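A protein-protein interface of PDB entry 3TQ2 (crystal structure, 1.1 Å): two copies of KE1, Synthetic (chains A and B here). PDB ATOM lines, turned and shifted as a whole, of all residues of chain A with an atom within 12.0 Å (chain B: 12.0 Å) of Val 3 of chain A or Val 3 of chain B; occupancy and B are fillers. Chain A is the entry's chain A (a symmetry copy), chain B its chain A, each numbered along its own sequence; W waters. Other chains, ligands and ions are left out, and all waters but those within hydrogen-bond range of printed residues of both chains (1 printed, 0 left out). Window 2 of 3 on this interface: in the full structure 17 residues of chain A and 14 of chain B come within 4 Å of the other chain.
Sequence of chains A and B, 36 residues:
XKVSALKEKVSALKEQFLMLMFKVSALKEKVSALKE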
ATOM      1  C   ACE A   1     -15.397  12.538 -15.986  1.00  0.00           C
ATOM      2  O   ACE A   1     -16.238  11.747 -15.370  1.00  0.00           O
ATOM      3  CH3 ACE A   1     -15.371  12.274 -17.426  1.00  0.00           C
ATOM      4  N   LYS A   2     -14.563  13.494 -15.465  1.00  0.00           N
ATOM      5  CA  LYS A   2     -13.738  14.468 -16.167  1.00  0.00           C
ATOM      6  C   LYS A   2     -12.662  13.862 -17.025  1.00  0.00           C
ATOM      7  O   LYS A   2     -12.373  14.333 -18.158  1.00  0.00           O
ATOM      8  CB  LYS A   2     -13.049  15.393 -15.139  1.00  0.00           C
ATOM      9  CG  LYS A   2     -13.881  16.596 -14.755  1.00  0.00           C
ATOM     10  CD  LYS A   2     -13.233  17.854 -15.339  1.00  0.00           C
ATOM     11  CE  LYS A   2     -13.309  17.827 -16.856  1.00  0.00           C
ATOM     12  NZ  LYS A   2     -13.115  19.225 -17.428  1.00  0.00           N
ATOM     13  N   VAL A   3     -12.059  12.774 -16.548  1.00  0.00           N
ATOM     14  CA  VAL A   3     -10.960  12.160 -17.322  1.00  0.00           C
ATOM     15  C   VAL A   3     -11.582  11.557 -18.566  1.00  0.00           C
ATOM     16  O   VAL A   3     -10.996  11.686 -19.648  1.00  0.00           O
ATOM     17  CB  VAL A   3     -10.141  11.174 -16.488  1.00  0.00           C
ATOM     18  CG1 VAL A   3      -9.033  10.565 -17.322  1.00  0.00           C
ATOM     19  CG2 VAL A   3      -9.522  11.887 -15.277  1.00  0.00           C
ATOM     20  N   SER A   4     -12.750  10.934 -18.425  1.00  0.00           N
ATOM     21  CA  SER A   4     -13.431  10.355 -19.586  1.00  0.00           C
ATOM     22  C   SER A   4     -13.798  11.463 -20.581  1.00  0.00           C
ATOM     23  O   SER A   4     -13.556  11.215 -21.778  1.00  0.00           O
ATOM     24  CB  SER A   4     -14.666   9.557 -19.138  1.00  0.00           C
ATOM     25  OG  SER A   4     -14.251   8.522 -18.253  1.00  0.00           O
ATOM     26  N   ALA A   5     -14.311  12.551 -20.126  1.00  0.00           N
ATOM     27  CA  ALA A   5     -14.710  13.599 -21.084  1.00  0.00           C
ATOM     28  C   ALA A   5     -13.457  14.009 -21.856  1.00  0.00           C
ATOM     29  O   ALA A   5     -13.550  14.153 -23.109  1.00  0.00           O
ATOM     30  CB  ALA A   5     -15.409  14.724 -20.382  1.00  0.00           C
ATOM     31  N   LEU A   6     -12.347  14.138 -21.167  1.00  0.00           N
ATOM     32  CA  LEU A   6     -11.089  14.587 -21.738  1.00  0.00           C
ATOM     33  C   LEU A   6     -10.567  13.609 -22.761  1.00  0.00           C
ATOM     34  O   LEU A   6     -10.073  14.019 -23.862  1.00  0.00           O
ATOM     35  CB  LEU A   6      -9.991  14.778 -20.658  1.00  0.00           C
ATOM     36  CG  LEU A   6      -9.259  16.123 -20.810  1.00  0.00           C
ATOM     37  CD1 LEU A   6     -10.260  17.243 -20.570  1.00  0.00           C
ATOM     38  CD2 LEU A   6      -8.052  16.234 -19.894  1.00  0.00           C
ATOM     39  N   LYS A   7     -10.618  12.315 -22.470  1.00  0.00           N
ATOM     40  CA  LYS A   7     -10.185  11.293 -23.414  1.00  0.00           C
ATOM     41  C   LYS A   7     -11.022  11.426 -24.693  1.00  0.00           C
ATOM     42  O   LYS A   7     -10.390  11.319 -25.767  1.00  0.00           O
ATOM     43  CB  LYS A   7     -10.171   9.927 -22.747  1.00  0.00           C
ATOM     44  CG  LYS A   7     -11.482   9.203 -22.537  1.00  0.00           C
ATOM     45  CD  LYS A   7     -11.223   7.839 -21.904  1.00  0.00           C
ATOM     46  CE  LYS A   7     -11.859   6.729 -22.720  1.00  0.00           C
ATOM     47  NZ  LYS A   7     -10.825   5.755 -23.157  1.00  0.00           N
ATOM     48  N   GLU A   8     -12.292  11.698 -24.656  1.00  0.00           N
ATOM     49  CA  GLU A   8     -13.121  11.769 -25.870  1.00  0.00           C
ATOM     50  C   GLU A   8     -12.779  13.016 -26.673  1.00  0.00           C
ATOM     51  O   GLU A   8     -12.803  12.947 -27.914  1.00  0.00           O
ATOM     52  CB  GLU A   8     -14.598  11.804 -25.483  1.00  0.00           C
ATOM     53  CG  GLU A   8     -15.371  10.540 -25.250  1.00  0.00           C
ATOM     54  CD  GLU A   8     -14.804   9.513 -24.303  1.00  0.00           C
ATOM     55  OE1 GLU A   8     -15.223   9.438 -23.130  1.00  0.00           O
ATOM     56  OE2 GLU A   8     -13.913   8.738 -24.736  1.00  0.00           O
ATOM     57  N   LYS A   9     -12.474  14.077 -25.954  1.00  0.00           N
ATOM     58  CA  LYS A   9     -12.103  15.353 -26.569  1.00  0.00           C
ATOM     59  C   LYS A   9     -10.781  15.129 -27.309  1.00  0.00           C
ATOM     60  O   LYS A   9     -10.684  15.627 -28.453  1.00  0.00           O
ATOM     61  CB  LYS A   9     -12.009  16.436 -25.516  1.00  0.00           C
ATOM     62  CG  LYS A   9     -13.075  17.473 -25.378  1.00  0.00           C
ATOM     63  CD  LYS A   9     -14.476  16.996 -25.069  1.00  0.00           C
ATOM     64  CE  LYS A   9     -15.411  18.169 -24.769  1.00  0.00           C
ATOM     65  NZ  LYS A   9     -16.635  18.203 -25.628  1.00  0.00           N
ATOM     66  N   VAL A  10      -9.841  14.415 -26.693  1.00  0.00           N
ATOM     67  CA  VAL A  10      -8.552  14.154 -27.370  1.00  0.00           C
ATOM     68  C   VAL A  10      -8.768  13.213 -28.556  1.00  0.00           C
ATOM     69  O   VAL A  10      -8.132  13.390 -29.627  1.00  0.00           O
ATOM     70  CB  VAL A  10      -7.577  13.603 -26.315  1.00  0.00           C
ATOM     71  CG1 VAL A  10      -6.322  13.059 -26.976  1.00  0.00           C
ATOM     72  CG2 VAL A  10      -7.237  14.714 -25.338  1.00  0.00           C
ATOM     73  N   SER A  11      -9.644  12.228 -28.415  1.00  0.00           N
ATOM     74  CA  SER A  11      -9.961  11.355 -29.538  1.00  0.00           C
ATOM     75  C   SER A  11     -10.478  12.103 -30.745  1.00  0.00           C
ATOM     76  O   SER A  11     -10.040  11.817 -31.866  1.00  0.00           O
ATOM     77  CB  SER A  11     -11.005  10.345 -29.009  1.00  0.00           C
ATOM     78  OG  SER A  11     -10.320   9.458 -28.121  1.00  0.00           O
ATOM     79  N   ALA A  12     -11.389  13.022 -30.491  1.00  0.00           N
ATOM     80  CA  ALA A  12     -12.002  13.757 -31.596  1.00  0.00           C
ATOM     81  C   ALA A  12     -10.956  14.677 -32.199  1.00  0.00           C
ATOM     82  O   ALA A  12     -10.856  14.863 -33.432  1.00  0.00           O
ATOM     83  CB  ALA A  12     -13.255  14.441 -31.089  1.00  0.00           C
ATOM     84  N   LYS A  14      -7.686  14.091 -32.286  1.00  0.00           N
ATOM     85  CA  LYS A  14      -6.813  13.298 -33.144  1.00  0.00           C
ATOM     86  C   LYS A  14      -7.412  12.997 -34.515  1.00  0.00           C
ATOM     87  O   LYS A  14      -6.713  12.953 -35.546  1.00  0.00           O
ATOM     88  CB  LYS A  14      -6.536  11.954 -32.446  1.00  0.00           C
ATOM     89  CG  LYS A  14      -5.307  11.877 -31.575  1.00  0.00           C
ATOM     90  CD  LYS A  14      -5.618  11.957 -30.084  1.00  0.00           C
ATOM     91  CE  LYS A  14      -4.342  11.766 -29.265  1.00  0.00           C
ATOM     92  NZ  LYS A  14      -3.867  13.058 -28.689  1.00  0.00           N
ATOM     93  C   ACE B   1      -3.169   5.862 -16.301  1.00  0.00           C
ATOM     94  O   ACE B   1      -2.534   5.170 -15.390  1.00  0.00           O
ATOM     95  CH3 ACE B   1      -2.241   6.451 -17.269  1.00  0.00           C
ATOM     96  N   LYS B   2      -4.511   6.116 -16.420  1.00  0.00           N
ATOM     97  CA  LYS B   2      -5.226   6.762 -17.513  1.00  0.00           C
ATOM     98  C   LYS B   2      -4.838   8.198 -17.740  1.00  0.00           C
ATOM     99  O   LYS B   2      -4.720   8.676 -18.899  1.00  0.00           O
ATOM    100  CB  LYS B   2      -6.744   6.728 -17.225  1.00  0.00           C
ATOM    101  CG  LYS B   2      -7.426   5.472 -17.720  1.00  0.00           C
ATOM    102  CD  LYS B   2      -8.324   5.830 -18.906  1.00  0.00           C
ATOM    103  CE  LYS B   2      -7.478   6.277 -20.087  1.00  0.00           C
ATOM    104  NZ  LYS B   2      -8.275   6.185 -21.382  1.00  0.00           N
ATOM    105  N   VAL B   3      -4.583   8.926 -16.655  1.00  0.00           N
ATOM    106  CA  VAL B   3      -4.244  10.356 -16.808  1.00  0.00           C
ATOM    107  C   VAL B   3      -2.876  10.416 -17.460  1.00  0.00           C
ATOM    108  O   VAL B   3      -2.676  11.254 -18.349  1.00  0.00           O
ATOM    109  CB  VAL B   3      -4.347  11.124 -15.491  1.00  0.00           C
ATOM    110  CG1 VAL B   3      -3.985  12.581 -15.694  1.00  0.00           C
ATOM    111  CG2 VAL B   3      -5.776  11.037 -14.933  1.00  0.00           C
ATOM    112  N   SER B   4      -1.964   9.539 -17.048  1.00  0.00           N
ATOM    113  CA  SER B   4      -0.630   9.512 -17.652  1.00  0.00           C
ATOM    114  C   SER B   4      -0.739   9.157 -19.141  1.00  0.00           C
ATOM    115  O   SER B   4      -0.048   9.850 -19.913  1.00  0.00           O
ATOM    116  CB  SER B   4       0.280   8.529 -16.897  1.00  0.00           C
ATOM    117  OG  SER B   4       0.371   8.939 -15.536  1.00  0.00           O
ATOM    118  N   ALA B   5      -1.522   8.198 -19.487  1.00  0.00           N
ATOM    119  CA  ALA B   5      -1.593   7.822 -20.912  1.00  0.00           C
ATOM    120  C   ALA B   5      -2.062   9.055 -21.683  1.00  0.00           C
ATOM    121  O   ALA B   5      -1.470   9.343 -22.763  1.00  0.00           O
ATOM    122  CB  ALA B   5      -2.446   6.603 -21.100  1.00  0.00           C
ATOM    123  N   LEU B   6      -3.025   9.765 -21.143  1.00  0.00           N
ATOM    124  CA  LEU B   6      -3.629  10.923 -21.780  1.00  0.00           C
ATOM    125  C   LEU B   6      -2.634  12.044 -21.947  1.00  0.00           C
ATOM    126  O   LEU B   6      -2.583  12.714 -23.029  1.00  0.00           O
ATOM    127  CB  LEU B   6      -4.835  11.474 -20.971  1.00  0.00           C
ATOM    128  CG  LEU B   6      -6.060  11.733 -21.866  1.00  0.00           C
ATOM    129  CD1 LEU B   6      -6.529  10.403 -22.435  1.00  0.00           C
ATOM    130  CD2 LEU B   6      -7.172  12.459 -21.131  1.00  0.00           C
ATOM    131  N   LYS B   7      -1.832  12.323 -20.926  1.00  0.00           N
ATOM    132  CA  LYS B   7      -0.805  13.354 -21.010  1.00  0.00           C
ATOM    133  C   LYS B   7       0.151  12.995 -22.156  1.00  0.00           C
ATOM    134  O   LYS B   7       0.496  13.947 -22.891  1.00  0.00           O
ATOM    135  CB  LYS B   7      -0.177  13.589 -19.646  1.00  0.00           C
ATOM    136  CG  LYS B   7       0.838  12.594 -19.128  1.00  0.00           C
ATOM    137  CD  LYS B   7       1.368  13.056 -17.775  1.00  0.00           C
ATOM    138  CE  LYS B   7       2.885  13.127 -17.779  1.00  0.00           C
ATOM    139  NZ  LYS B   7       3.336  14.504 -17.452  1.00  0.00           N
ATOM    140  N   GLU B   8       0.521  11.771 -22.382  1.00  0.00           N
ATOM    141  CA  GLU B   8       1.484  11.418 -23.438  1.00  0.00           C
ATOM    142  C   GLU B   8       0.848  11.582 -24.811  1.00  0.00           C
ATOM    143  O   GLU B   8       1.555  11.998 -25.746  1.00  0.00           O
ATOM    144  CB  GLU B   8       1.937   9.971 -23.259  1.00  0.00           C
ATOM    145  CG  GLU B   8       3.080   9.621 -22.354  1.00  0.00           C
ATOM    146  CD  GLU B   8       3.064  10.142 -20.939  1.00  0.00           C
ATOM    147  OE1 GLU B   8       2.700   9.404 -20.000  1.00  0.00           O
ATOM    148  OE2 GLU B   8       3.436  11.327 -20.741  1.00  0.00           O
ATOM    149  N   LYS B   9      -0.430  11.267 -24.877  1.00  0.00           N
ATOM    150  CA  LYS B   9      -1.197  11.385 -26.119  1.00  0.00           C
ATOM    151  C   LYS B   9      -1.260  12.875 -26.471  1.00  0.00           C
ATOM    152  O   LYS B   9      -1.066  13.180 -27.668  1.00  0.00           O
ATOM    153  CB  LYS B   9      -2.567  10.765 -25.950  1.00  0.00           C
ATOM    154  CG  LYS B   9      -2.894   9.439 -26.553  1.00  0.00           C
ATOM    155  CD  LYS B   9      -2.067   8.252 -26.114  1.00  0.00           C
ATOM    156  CE  LYS B   9      -2.636   6.942 -26.665  1.00  0.00           C
ATOM    157  NZ  LYS B   9      -1.649   6.133 -27.446  1.00  0.00           N
ATOM    158  N   VAL B  10      -1.500  13.734 -25.481  1.00  0.00           N
ATOM    159  CA  VAL B  10      -1.554  15.184 -25.763  1.00  0.00           C
ATOM    160  C   VAL B  10      -0.160  15.695 -26.132  1.00  0.00           C
ATOM    161  O   VAL B  10      -0.022  16.557 -27.039  1.00  0.00           O
ATOM    162  CB  VAL B  10      -2.155  15.876 -24.528  1.00  0.00           C
ATOM    163  CG1 VAL B  10      -1.998  17.384 -24.625  1.00  0.00           C
ATOM    164  CG2 VAL B  10      -3.620  15.489 -24.418  1.00  0.00           C
ATOM    165  N   SER B  11       0.877  15.194 -25.478  1.00  0.00           N
ATOM    166  CA  SER B  11       2.236  15.571 -25.846  1.00  0.00           C
ATOM    167  C   SER B  11       2.566  15.273 -27.291  1.00  0.00           C
ATOM    168  O   SER B  11       3.154  16.126 -27.966  1.00  0.00           O
ATOM    169  CB  SER B  11       3.168  14.800 -24.884  1.00  0.00           C
ATOM    170  OG  SER B  11       3.028  15.400 -23.592  1.00  0.00           O
ATOM    171  N   ALA B  12       2.192  14.083 -27.720  1.00  0.00           N
ATOM    172  CA  ALA B  12       2.521  13.669 -29.083  1.00  0.00           C
ATOM    173  C   ALA B  12       1.693  14.495 -30.049  1.00  0.00           C
ATOM    174  O   ALA B  12       2.155  14.935 -31.124  1.00  0.00           O
ATOM    175  CB  ALA B  12       2.343  12.169 -29.191  1.00  0.00           C
ATOM    176  N   LYS B  14       0.653  17.609 -29.528  1.00  0.00           N
ATOM    177  CA  LYS B  14       1.268  18.925 -29.655  1.00  0.00           C
ATOM    178  C   LYS B  14       2.474  18.951 -30.589  1.00  0.00           C
ATOM    179  O   LYS B  14       2.721  19.926 -31.324  1.00  0.00           O
ATOM    180  CB  LYS B  14       1.743  19.376 -28.261  1.00  0.00           C
ATOM    181  CG  LYS B  14       0.780  20.198 -27.443  1.00  0.00           C
ATOM    182  CD  LYS B  14       0.088  19.400 -26.342  1.00  0.00           C
ATOM    183  CE  LYS B  14      -0.788  20.318 -25.492  1.00  0.00           C
ATOM    184  NZ  LYS B  14      -2.236  20.126 -25.800  1.00  0.00           N
HETATM  185  O   HOH W   1     -10.547   5.506 -20.577  1.00  0.00           O
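The side-chain amino group of Lys 14 of chain A lies within hydrogen-bond range of the backbone carbonyl oxygen of Lys 9 of chain B. The side-chain amino group of Lys 2 of chain B lies close to the side-chain amino group of Lys 7 of chain A.
Val 3 of chain A touches its own counterpart, Val 3 of chain B. Leu 6 of chain B touches its own counterpart, Leu 6 of chain A. Lys 7 of chain A touches Leu 6 of chain B, but with the chains exchanged Leu 6 of chain A does not touch Lys 7 of chain B (7.4 Å). Val 10 of chain A touches its own counterpart, Val 10 of chain B. Positions printed for both chains: 1, 2, 3, 4, 5, 6, 7, 8, 9, 10, 11, 12 and 14.
Water W1 bridges NZ of Lys 2 of chain B and NZ of Lys 7 of chain A.
Along chain A the printed residues that touch a printed residue of chain B span positions 3 to 14. Of the 13 printed residues of chain B, 5 touch a printed residue of chain A. Hydrophobic or aromatic side chains of chain B that line the printed part of chain A: Val 3, Leu 6 and Val 10.
Among the printed residues, merely in contact across the chains: Val 3 of chain A with Val 3 of chain B, Leu 6 of chain A with Leu 6 of chain B, Lys 7 of chain A with Leu 6 of chain B and Val 10 of chain A with Val 10 of chain B.
No residue of chain B comes within 4 Å of ACE 1 of chain A. No residue of chain B comes within 4 Å of Lys 2 of chain A. Val 3 of chain A touches one residue of chain B. No residue of chain B comes within 4 Å of Ala 5 of chain A. Of chain B, only Leu 6 (3.7 Å) comes within 4 Å of Leu 6 of chain A. Ala 12 of chain A touches none of the printed residues of chain B. Of the printed residues of chain B, Lys 14 of chain A touches Lys 9 (3.0 Å). No residue of chain A comes within 4 Å of ACE 1 of chain B. Lys 2 of chain B touches just one residue of chain A: Lys 7 (3.1 Å). Val 3 of chain B touches just one residue of chain A: Val 3 (3.9 Å). No residue of chain A comes within 4 Å of Ser 4 of chain B. No residue of chain A comes within 4 Å of Ala 5 of chain B. Leu 6 of chain B touches two residues of chain A. No residue of chain A comes within 4 Å of Lys 7 of chain B. Printed residues of chain A within 4 Å of Lys 9 of chain B: Lys 14 (3.0 Å). Of the printed residues of chain A, Val 10 of chain B touches Val 10 (3.8 Å). The nearest residue of chain A that does not touch Val 3 of chain B is Leu 6 of chain A (6.9 Å).
The side-chain hydroxyl (OG) of Ser 11 of chain A is in hydrogen-bond range of the backbone carbonyl oxygen (O) of Lys 7 of chain A (3.0 Å).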
